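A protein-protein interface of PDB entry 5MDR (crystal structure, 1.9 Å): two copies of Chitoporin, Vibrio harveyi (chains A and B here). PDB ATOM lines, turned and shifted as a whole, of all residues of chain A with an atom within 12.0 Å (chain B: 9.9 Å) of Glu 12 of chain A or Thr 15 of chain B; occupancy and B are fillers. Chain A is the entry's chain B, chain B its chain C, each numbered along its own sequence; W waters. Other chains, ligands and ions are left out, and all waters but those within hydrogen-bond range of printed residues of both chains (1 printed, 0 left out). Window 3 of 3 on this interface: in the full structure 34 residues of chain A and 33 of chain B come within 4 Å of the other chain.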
ATOM      1  N   GLU A  12     -14.460  20.700  20.950  1.00  0.00           N
ATOM      2  CA  GLU A  12     -15.136  19.392  21.194  1.00  0.00           C
ATOM      3  C   GLU A  12     -15.353  18.592  19.894  1.00  0.00           C
ATOM      4  O   GLU A  12     -15.035  17.405  19.856  1.00  0.00           O
ATOM      5  CB  GLU A  12     -16.461  19.619  21.902  1.00  0.00           C
ATOM      6  CG  GLU A  12     -17.102  18.346  22.439  1.00  0.00           C
ATOM      7  CD  GLU A  12     -18.617  18.436  22.511  1.00  0.00           C
ATOM      8  OE1 GLU A  12     -19.236  17.467  22.998  1.00  0.00           O
ATOM      9  OE2 GLU A  12     -19.201  19.456  22.084  1.00  0.00           O
ATOM     10  N   TYR A  13     -15.879  19.238  18.851  1.00  0.00           N
ATOM     11  CA  TYR A  13     -15.998  18.614  17.527  1.00  0.00           C
ATOM     12  C   TYR A  13     -14.689  18.686  16.755  1.00  0.00           C
ATOM     13  O   TYR A  13     -13.990  19.691  16.795  1.00  0.00           O
ATOM     14  CB  TYR A  13     -17.105  19.248  16.708  1.00  0.00           C
ATOM     15  CG  TYR A  13     -18.470  18.932  17.265  1.00  0.00           C
ATOM     16  CD1 TYR A  13     -19.053  17.685  17.048  1.00  0.00           C
ATOM     17  CD2 TYR A  13     -19.165  19.860  18.030  1.00  0.00           C
ATOM     18  CE1 TYR A  13     -20.307  17.390  17.565  1.00  0.00           C
ATOM     19  CE2 TYR A  13     -20.419  19.571  18.552  1.00  0.00           C
ATOM     20  CZ  TYR A  13     -20.979  18.330  18.313  1.00  0.00           C
ATOM     21  OH  TYR A  13     -22.214  18.035  18.830  1.00  0.00           O
ATOM     22  N   LEU A  14     -14.375  17.625  16.027  1.00  0.00           N
ATOM     23  CA  LEU A  14     -13.075  17.492  15.370  1.00  0.00           C
ATOM     24  C   LEU A  14     -13.085  18.028  13.943  1.00  0.00           C
ATOM     25  O   LEU A  14     -14.091  17.926  13.239  1.00  0.00           O
ATOM     26  CB  LEU A  14     -12.645  16.020  15.342  1.00  0.00           C
ATOM     27  CG  LEU A  14     -12.655  15.301  16.686  1.00  0.00           C
ATOM     28  CD1 LEU A  14     -12.391  13.812  16.503  1.00  0.00           C
ATOM     29  CD2 LEU A  14     -11.643  15.919  17.630  1.00  0.00           C
ATOM     30  N   THR A  15     -11.945  18.588  13.529  1.00  0.00           N
ATOM     31  CA  THR A  15     -11.663  18.921  12.122  1.00  0.00           C
ATOM     32  C   THR A  15     -10.417  18.182  11.690  1.00  0.00           C
ATOM     33  O   THR A  15      -9.763  17.524  12.507  1.00  0.00           O
ATOM     34  CB  THR A  15     -11.434  20.442  11.914  1.00  0.00           C
ATOM     35  OG1 THR A  15     -10.216  20.842  12.558  1.00  0.00           O
ATOM     36  CG2 THR A  15     -12.602  21.258  12.479  1.00  0.00           C
ATOM     37  N   LYS A  16     -10.097  18.284  10.404  1.00  0.00           N
ATOM     38  CA  LYS A  16      -8.834  17.760   9.838  1.00  0.00           C
ATOM     39  C   LYS A  16      -7.621  18.245  10.651  1.00  0.00           C
ATOM     40  O   LYS A  16      -6.707  17.462  10.947  1.00  0.00           O
ATOM     41  CB  LYS A  16      -8.672  18.189   8.375  1.00  0.00           C
ATOM     42  CG  LYS A  16      -7.851  17.236   7.520  1.00  0.00           C
ATOM     43  CD  LYS A  16      -8.728  16.349   6.643  1.00  0.00           C
ATOM     44  CE  LYS A  16      -7.912  15.532   5.647  1.00  0.00           C
ATOM     45  NZ  LYS A  16      -7.052  14.520   6.313  1.00  0.00           N
ATOM     46  N   ASP A  17      -7.673  19.512  11.064  1.00  0.00           N
ATOM     47  CA  ASP A  17      -6.647  20.135  11.912  1.00  0.00           C
ATOM     48  C   ASP A  17      -6.552  19.621  13.338  1.00  0.00           C
ATOM     49  O   ASP A  17      -5.613  19.968  14.039  1.00  0.00           O
ATOM     50  CB  ASP A  17      -6.867  21.662  11.990  1.00  0.00           C
ATOM     51  CG  ASP A  17      -6.727  22.345  10.649  1.00  0.00           C
ATOM     52  OD1 ASP A  17      -6.113  21.765   9.726  1.00  0.00           O
ATOM     53  OD2 ASP A  17      -7.217  23.481  10.522  1.00  0.00           O
ATOM     54  N   SER A  18      -7.524  18.848  13.803  1.00  0.00           N
ATOM     55  CA  SER A  18      -7.411  18.200  15.098  1.00  0.00           C
ATOM     56  C   SER A  18      -6.341  17.095  15.125  1.00  0.00           C
ATOM     57  O   SER A  18      -5.938  16.695  16.199  1.00  0.00           O
ATOM     58  CB  SER A  18      -8.748  17.578  15.497  1.00  0.00           C
ATOM     59  OG  SER A  18      -9.808  18.525  15.399  1.00  0.00           O
ATOM     60  N   PHE A  19      -5.938  16.561  13.978  1.00  0.00           N
ATOM     61  CA  PHE A  19      -4.995  15.450  13.931  1.00  0.00           C
ATOM     62  C   PHE A  19      -3.633  15.916  13.433  1.00  0.00           C
ATOM     63  O   PHE A  19      -3.565  16.783  12.579  1.00  0.00           O
ATOM     64  CB  PHE A  19      -5.522  14.356  13.009  1.00  0.00           C
ATOM     65  CG  PHE A  19      -6.755  13.691  13.533  1.00  0.00           C
ATOM     66  CD1 PHE A  19      -6.655  12.574  14.345  1.00  0.00           C
ATOM     67  CD2 PHE A  19      -8.011  14.224  13.280  1.00  0.00           C
ATOM     68  CE1 PHE A  19      -7.803  11.959  14.854  1.00  0.00           C
ATOM     69  CE2 PHE A  19      -9.156  13.624  13.789  1.00  0.00           C
ATOM     70  CZ  PHE A  19      -9.057  12.501  14.582  1.00  0.00           C
ATOM     71  N   TYR A  21      -1.501  13.585  12.156  1.00  0.00           N
ATOM     72  CA  TYR A  21      -1.097  12.514  11.290  1.00  0.00           C
ATOM     73  C   TYR A  21      -2.292  12.163  10.411  1.00  0.00           C
ATOM     74  O   TYR A  21      -3.435  12.537  10.700  1.00  0.00           O
ATOM     75  CB  TYR A  21      -0.698  11.242  12.087  1.00  0.00           C
ATOM     76  CG  TYR A  21      -1.882  10.632  12.769  1.00  0.00           C
ATOM     77  CD1 TYR A  21      -2.336  11.136  13.967  1.00  0.00           C
ATOM     78  CD2 TYR A  21      -2.605   9.600  12.167  1.00  0.00           C
ATOM     79  CE1 TYR A  21      -3.480  10.602  14.584  1.00  0.00           C
ATOM     80  CE2 TYR A  21      -3.751   9.052  12.779  1.00  0.00           C
ATOM     81  CZ  TYR A  21      -4.183   9.562  13.975  1.00  0.00           C
ATOM     82  OH  TYR A  21      -5.312   9.058  14.559  1.00  0.00           O
ATOM     83  N   GLU B  12     -23.531  11.943  14.452  1.00  0.00           N
ATOM     84  CA  GLU B  12     -22.960  12.023  13.075  1.00  0.00           C
ATOM     85  C   GLU B  12     -21.594  12.735  13.061  1.00  0.00           C
ATOM     86  O   GLU B  12     -20.649  12.235  12.446  1.00  0.00           O
ATOM     87  CB  GLU B  12     -23.938  12.725  12.148  1.00  0.00           C
ATOM     88  CG  GLU B  12     -23.581  12.619  10.671  1.00  0.00           C
ATOM     89  CD  GLU B  12     -24.093  13.791   9.849  1.00  0.00           C
ATOM     90  OE1 GLU B  12     -23.924  13.760   8.618  1.00  0.00           O
ATOM     91  OE2 GLU B  12     -24.650  14.748  10.425  1.00  0.00           O
ATOM     92  N   TYR B  13     -21.494  13.891  13.724  1.00  0.00           N
ATOM     93  CA  TYR B  13     -20.204  14.599  13.877  1.00  0.00           C
ATOM     94  C   TYR B  13     -19.381  14.020  15.022  1.00  0.00           C
ATOM     95  O   TYR B  13     -19.930  13.670  16.061  1.00  0.00           O
ATOM     96  CB  TYR B  13     -20.405  16.094  14.101  1.00  0.00           C
ATOM     97  CG  TYR B  13     -20.910  16.780  12.867  1.00  0.00           C
ATOM     98  CD1 TYR B  13     -20.046  17.077  11.812  1.00  0.00           C
ATOM     99  CD2 TYR B  13     -22.261  17.107  12.728  1.00  0.00           C
ATOM    100  CE1 TYR B  13     -20.505  17.697  10.663  1.00  0.00           C
ATOM    101  CE2 TYR B  13     -22.729  17.734  11.584  1.00  0.00           C
ATOM    102  CZ  TYR B  13     -21.846  18.016  10.555  1.00  0.00           C
ATOM    103  OH  TYR B  13     -22.303  18.623   9.420  1.00  0.00           O
ATOM    104  N   LEU B  14     -18.069  13.944  14.833  1.00  0.00           N
ATOM    105  CA  LEU B  14     -17.189  13.255  15.779  1.00  0.00           C
ATOM    106  C   LEU B  14     -16.629  14.188  16.834  1.00  0.00           C
ATOM    107  O   LEU B  14     -16.369  15.361  16.559  1.00  0.00           O
ATOM    108  CB  LEU B  14     -16.022  12.588  15.026  1.00  0.00           C
ATOM    109  CG  LEU B  14     -16.420  11.666  13.874  1.00  0.00           C
ATOM    110  CD1 LEU B  14     -15.183  11.223  13.105  1.00  0.00           C
ATOM    111  CD2 LEU B  14     -17.200  10.467  14.382  1.00  0.00           C
ATOM    112  N   THR B  15     -16.438  13.647  18.037  1.00  0.00           N
ATOM    113  CA  THR B  15     -15.669  14.302  19.105  1.00  0.00           C
ATOM    114  C   THR B  15     -14.523  13.385  19.505  1.00  0.00           C
ATOM    115  O   THR B  15     -14.440  12.259  19.028  1.00  0.00           O
ATOM    116  CB  THR B  15     -16.530  14.593  20.364  1.00  0.00           C
ATOM    117  OG1 THR B  15     -16.923  13.361  20.988  1.00  0.00           O
ATOM    118  CG2 THR B  15     -17.795  15.399  19.994  1.00  0.00           C
ATOM    119  N   LYS B  16     -13.664  13.878  20.396  1.00  0.00           N
ATOM    120  CA  LYS B  16     -12.607  13.085  21.020  1.00  0.00           C
ATOM    121  C   LYS B  16     -13.162  11.778  21.603  1.00  0.00           C
ATOM    122  O   LYS B  16     -12.557  10.706  21.441  1.00  0.00           O
ATOM    123  CB  LYS B  16     -11.906  13.887  22.125  1.00  0.00           C
ATOM    124  CG  LYS B  16     -10.446  13.497  22.367  1.00  0.00           C
ATOM    125  CD  LYS B  16      -9.476  14.486  21.715  1.00  0.00           C
ATOM    126  CE  LYS B  16      -8.027  14.220  22.110  1.00  0.00           C
ATOM    127  NZ  LYS B  16      -7.526  12.922  21.575  1.00  0.00           N
ATOM    128  N   ASP B  17     -14.332  11.875  22.232  1.00  0.00           N
ATOM    129  CA  ASP B  17     -15.050  10.725  22.798  1.00  0.00           C
ATOM    130  C   ASP B  17     -15.613   9.732  21.799  1.00  0.00           C
ATOM    131  O   ASP B  17     -16.065   8.673  22.203  1.00  0.00           O
ATOM    132  CB  ASP B  17     -16.233  11.211  23.661  1.00  0.00           C
ATOM    133  CG  ASP B  17     -15.793  12.007  24.871  1.00  0.00           C
ATOM    134  OD1 ASP B  17     -14.610  11.911  25.271  1.00  0.00           O
ATOM    135  OD2 ASP B  17     -16.640  12.738  25.425  1.00  0.00           O
ATOM    136  N   SER B  18     -15.648  10.068  20.512  1.00  0.00           N
ATOM    137  CA  SER B  18     -16.013   9.097  19.502  1.00  0.00           C
ATOM    138  C   SER B  18     -14.981   7.959  19.345  1.00  0.00           C
ATOM    139  O   SER B  18     -15.307   6.951  18.762  1.00  0.00           O
ATOM    140  CB  SER B  18     -16.188   9.777  18.146  1.00  0.00           C
ATOM    141  OG  SER B  18     -17.059  10.894  18.248  1.00  0.00           O
ATOM    142  N   PHE B  19     -13.735   8.158  19.782  1.00  0.00           N
ATOM    143  CA  PHE B  19     -12.669   7.192  19.565  1.00  0.00           C
ATOM    144  C   PHE B  19     -12.299   6.518  20.872  1.00  0.00           C
ATOM    145  O   PHE B  19     -12.320   7.140  21.904  1.00  0.00           O
ATOM    146  CB  PHE B  19     -11.430   7.887  18.981  1.00  0.00           C
ATOM    147  CG  PHE B  19     -11.636   8.416  17.583  1.00  0.00           C
ATOM    148  CD1 PHE B  19     -11.357   7.621  16.478  1.00  0.00           C
ATOM    149  CD2 PHE B  19     -12.173   9.693  17.375  1.00  0.00           C
ATOM    150  CE1 PHE B  19     -11.569   8.097  15.179  1.00  0.00           C
ATOM    151  CE2 PHE B  19     -12.380  10.172  16.091  1.00  0.00           C
ATOM    152  CZ  PHE B  19     -12.071   9.387  14.991  1.00  0.00           C
ATOM    153  N   SER B  20     -11.969   5.238  20.799  1.00  0.00           N
ATOM    154  CA  SER B  20     -11.500   4.471  21.949  1.00  0.00           C
ATOM    155  C   SER B  20      -9.990   4.318  21.976  1.00  0.00           C
ATOM    156  O   SER B  20      -9.456   3.527  22.763  1.00  0.00           O
ATOM    157  CB  SER B  20     -12.149   3.088  21.917  1.00  0.00           C
ATOM    158  OG  SER B  20     -13.542   3.230  21.992  1.00  0.00           O
ATOM    159  N   TYR B  21      -9.282   5.030  21.094  1.00  0.00           N
ATOM    160  CA  TYR B  21      -7.840   4.944  21.027  1.00  0.00           C
ATOM    161  C   TYR B  21      -7.335   6.312  20.588  1.00  0.00           C
ATOM    162  O   TYR B  21      -8.089   7.123  20.063  1.00  0.00           O
ATOM    163  CB  TYR B  21      -7.379   3.875  20.007  1.00  0.00           C
ATOM    164  CG  TYR B  21      -7.704   4.283  18.597  1.00  0.00           C
ATOM    165  CD1 TYR B  21      -8.960   4.072  18.081  1.00  0.00           C
ATOM    166  CD2 TYR B  21      -6.770   4.946  17.812  1.00  0.00           C
ATOM    167  CE1 TYR B  21      -9.298   4.506  16.814  1.00  0.00           C
ATOM    168  CE2 TYR B  21      -7.090   5.375  16.533  1.00  0.00           C
ATOM    169  CZ  TYR B  21      -8.354   5.177  16.042  1.00  0.00           C
ATOM    170  OH  TYR B  21      -8.681   5.620  14.768  1.00  0.00           O
HETATM  171  O   HOH W   1      -6.805   7.034  13.344  1.00  0.00           O
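Water W1 bridges the side-chain hydroxyl (OH) of Tyr 21 of chain B (2.7 Å) and the side-chain hydroxyl (OH) of Tyr 21 of chain A (2.8 Å).
OG of Ser 18 of chain B is in hydrogen-bond range of N of Thr 15 of chain B, at 2.8 Å.
The backbone NH of Asp 17 of chain B lies close to the side-chain hydroxyl of Thr 15 of chain B, 3.2 Å away.
Of chain B, only Thr 15 (3.2 Å) and Lys 16 (3.8 Å) come within 4 Å of Glu 12 of chain A.
Of chain B, only Tyr 13, Leu 14 and Thr 15 come within 4 Å of Tyr 13 of chain A.
Printed residues of chain B within 4 Å of Leu 14 of chain A: Leu 14 (3.1 Å), Thr 15 (3.6 Å), Lys 16 (3.99 Å) and Phe 19 (3.7 Å).
Glu 12 of chain B touches none of the printed residues of chain A.
Printed residues of chain A within 4 Å of Tyr 13 of chain B: Tyr 13 (3.6 Å).
Leu 14 of chain B touches just these residues of chain A: Tyr 13 (3.4 Å) and Leu 14 (3.1 Å).
Thr 15 of chain B touches just these residues of chain A: Glu 12 (3.2 Å), Tyr 13 (3.9 Å) and Leu 14 (3.6 Å).
Of the printed residues of chain A, Lys 16 of chain B touches Glu 12 and Leu 14.
No residue of chain A comes within 4 Å of Asp 17 of chain B.
Phe 19 of chain B touches just one residue of chain A: Leu 14 (3.7 Å).
The nearest residue of chain A that does not touch Thr 15 of chain B is Phe 19 of chain A (7.0 Å).
The backbone carbonyl oxygen (O) of Leu 14 of chain B sits at hydrogen-bond distance from the backbone NH (N) of Leu 14 of chain A, 3.1 Å away.
Among the printed residues, merely in contact across the chains: Glu 12 of chain A with Thr 15 of chain B (3.2 Å), Glu 12 of chain A with Lys 16 of chain B (3.8 Å), Tyr 13 of chain A with Tyr 13 of chain B (3.6 Å), Tyr 13 of chain A with Leu 14 of chain B (3.4 Å), Tyr 13 of chain A with Thr 15 of chain B (3.9 Å), Leu 14 of chain A with Thr 15 of chain B (3.6 Å), Leu 14 of chain A with Lys 16 of chain B (3.99 Å) and Leu 14 of chain A with Phe 19 of chain B (3.7 Å).
Of the 10 printed residues of chain B, 5 touch a printed residue of chain A.
Printed residues of chain B that touch a printed residue of chain A: Tyr 13, Leu 14, Thr 15, Lys 16 and Phe 19.
Along chain B the printed residues that touch a printed residue of chain A span positions 13 to 19.
Hydrophobic or aromatic side chains of chain A within 4 Å of the printed part of chain B: Tyr 13 and Leu 14.
Among the printed residues, 9 pairs touch across the chains.
Among the printed residues, no Asp or Glu carboxylate lies within 4 Å of a Lys or Arg side-chain nitrogen of the other chain.
Glu 12 of chain A touches Lys 16 of chain B, but with the chains exchanged Lys 16 of chain A does not touch Glu 12 of chain B (12.3 Å).
Tyr 13 of chain B touches its own counterpart, Tyr 13 of chain A.
Tyr 13 of chain A touches Leu 14 of chain B, but with the chains exchanged Leu 14 of chain A does not touch Tyr 13 of chain B (6.2 Å).
Leu 14 of chain A touches Thr 15 of chain B, but with the chains exchanged Thr 15 of chain A does not touch Leu 14 of chain B (6.3 Å).
9 positions are printed for both chains.
Of the 9 pairs that touch across the chains among the printed residues, 2 have their exchanged pair printed and touching as well.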
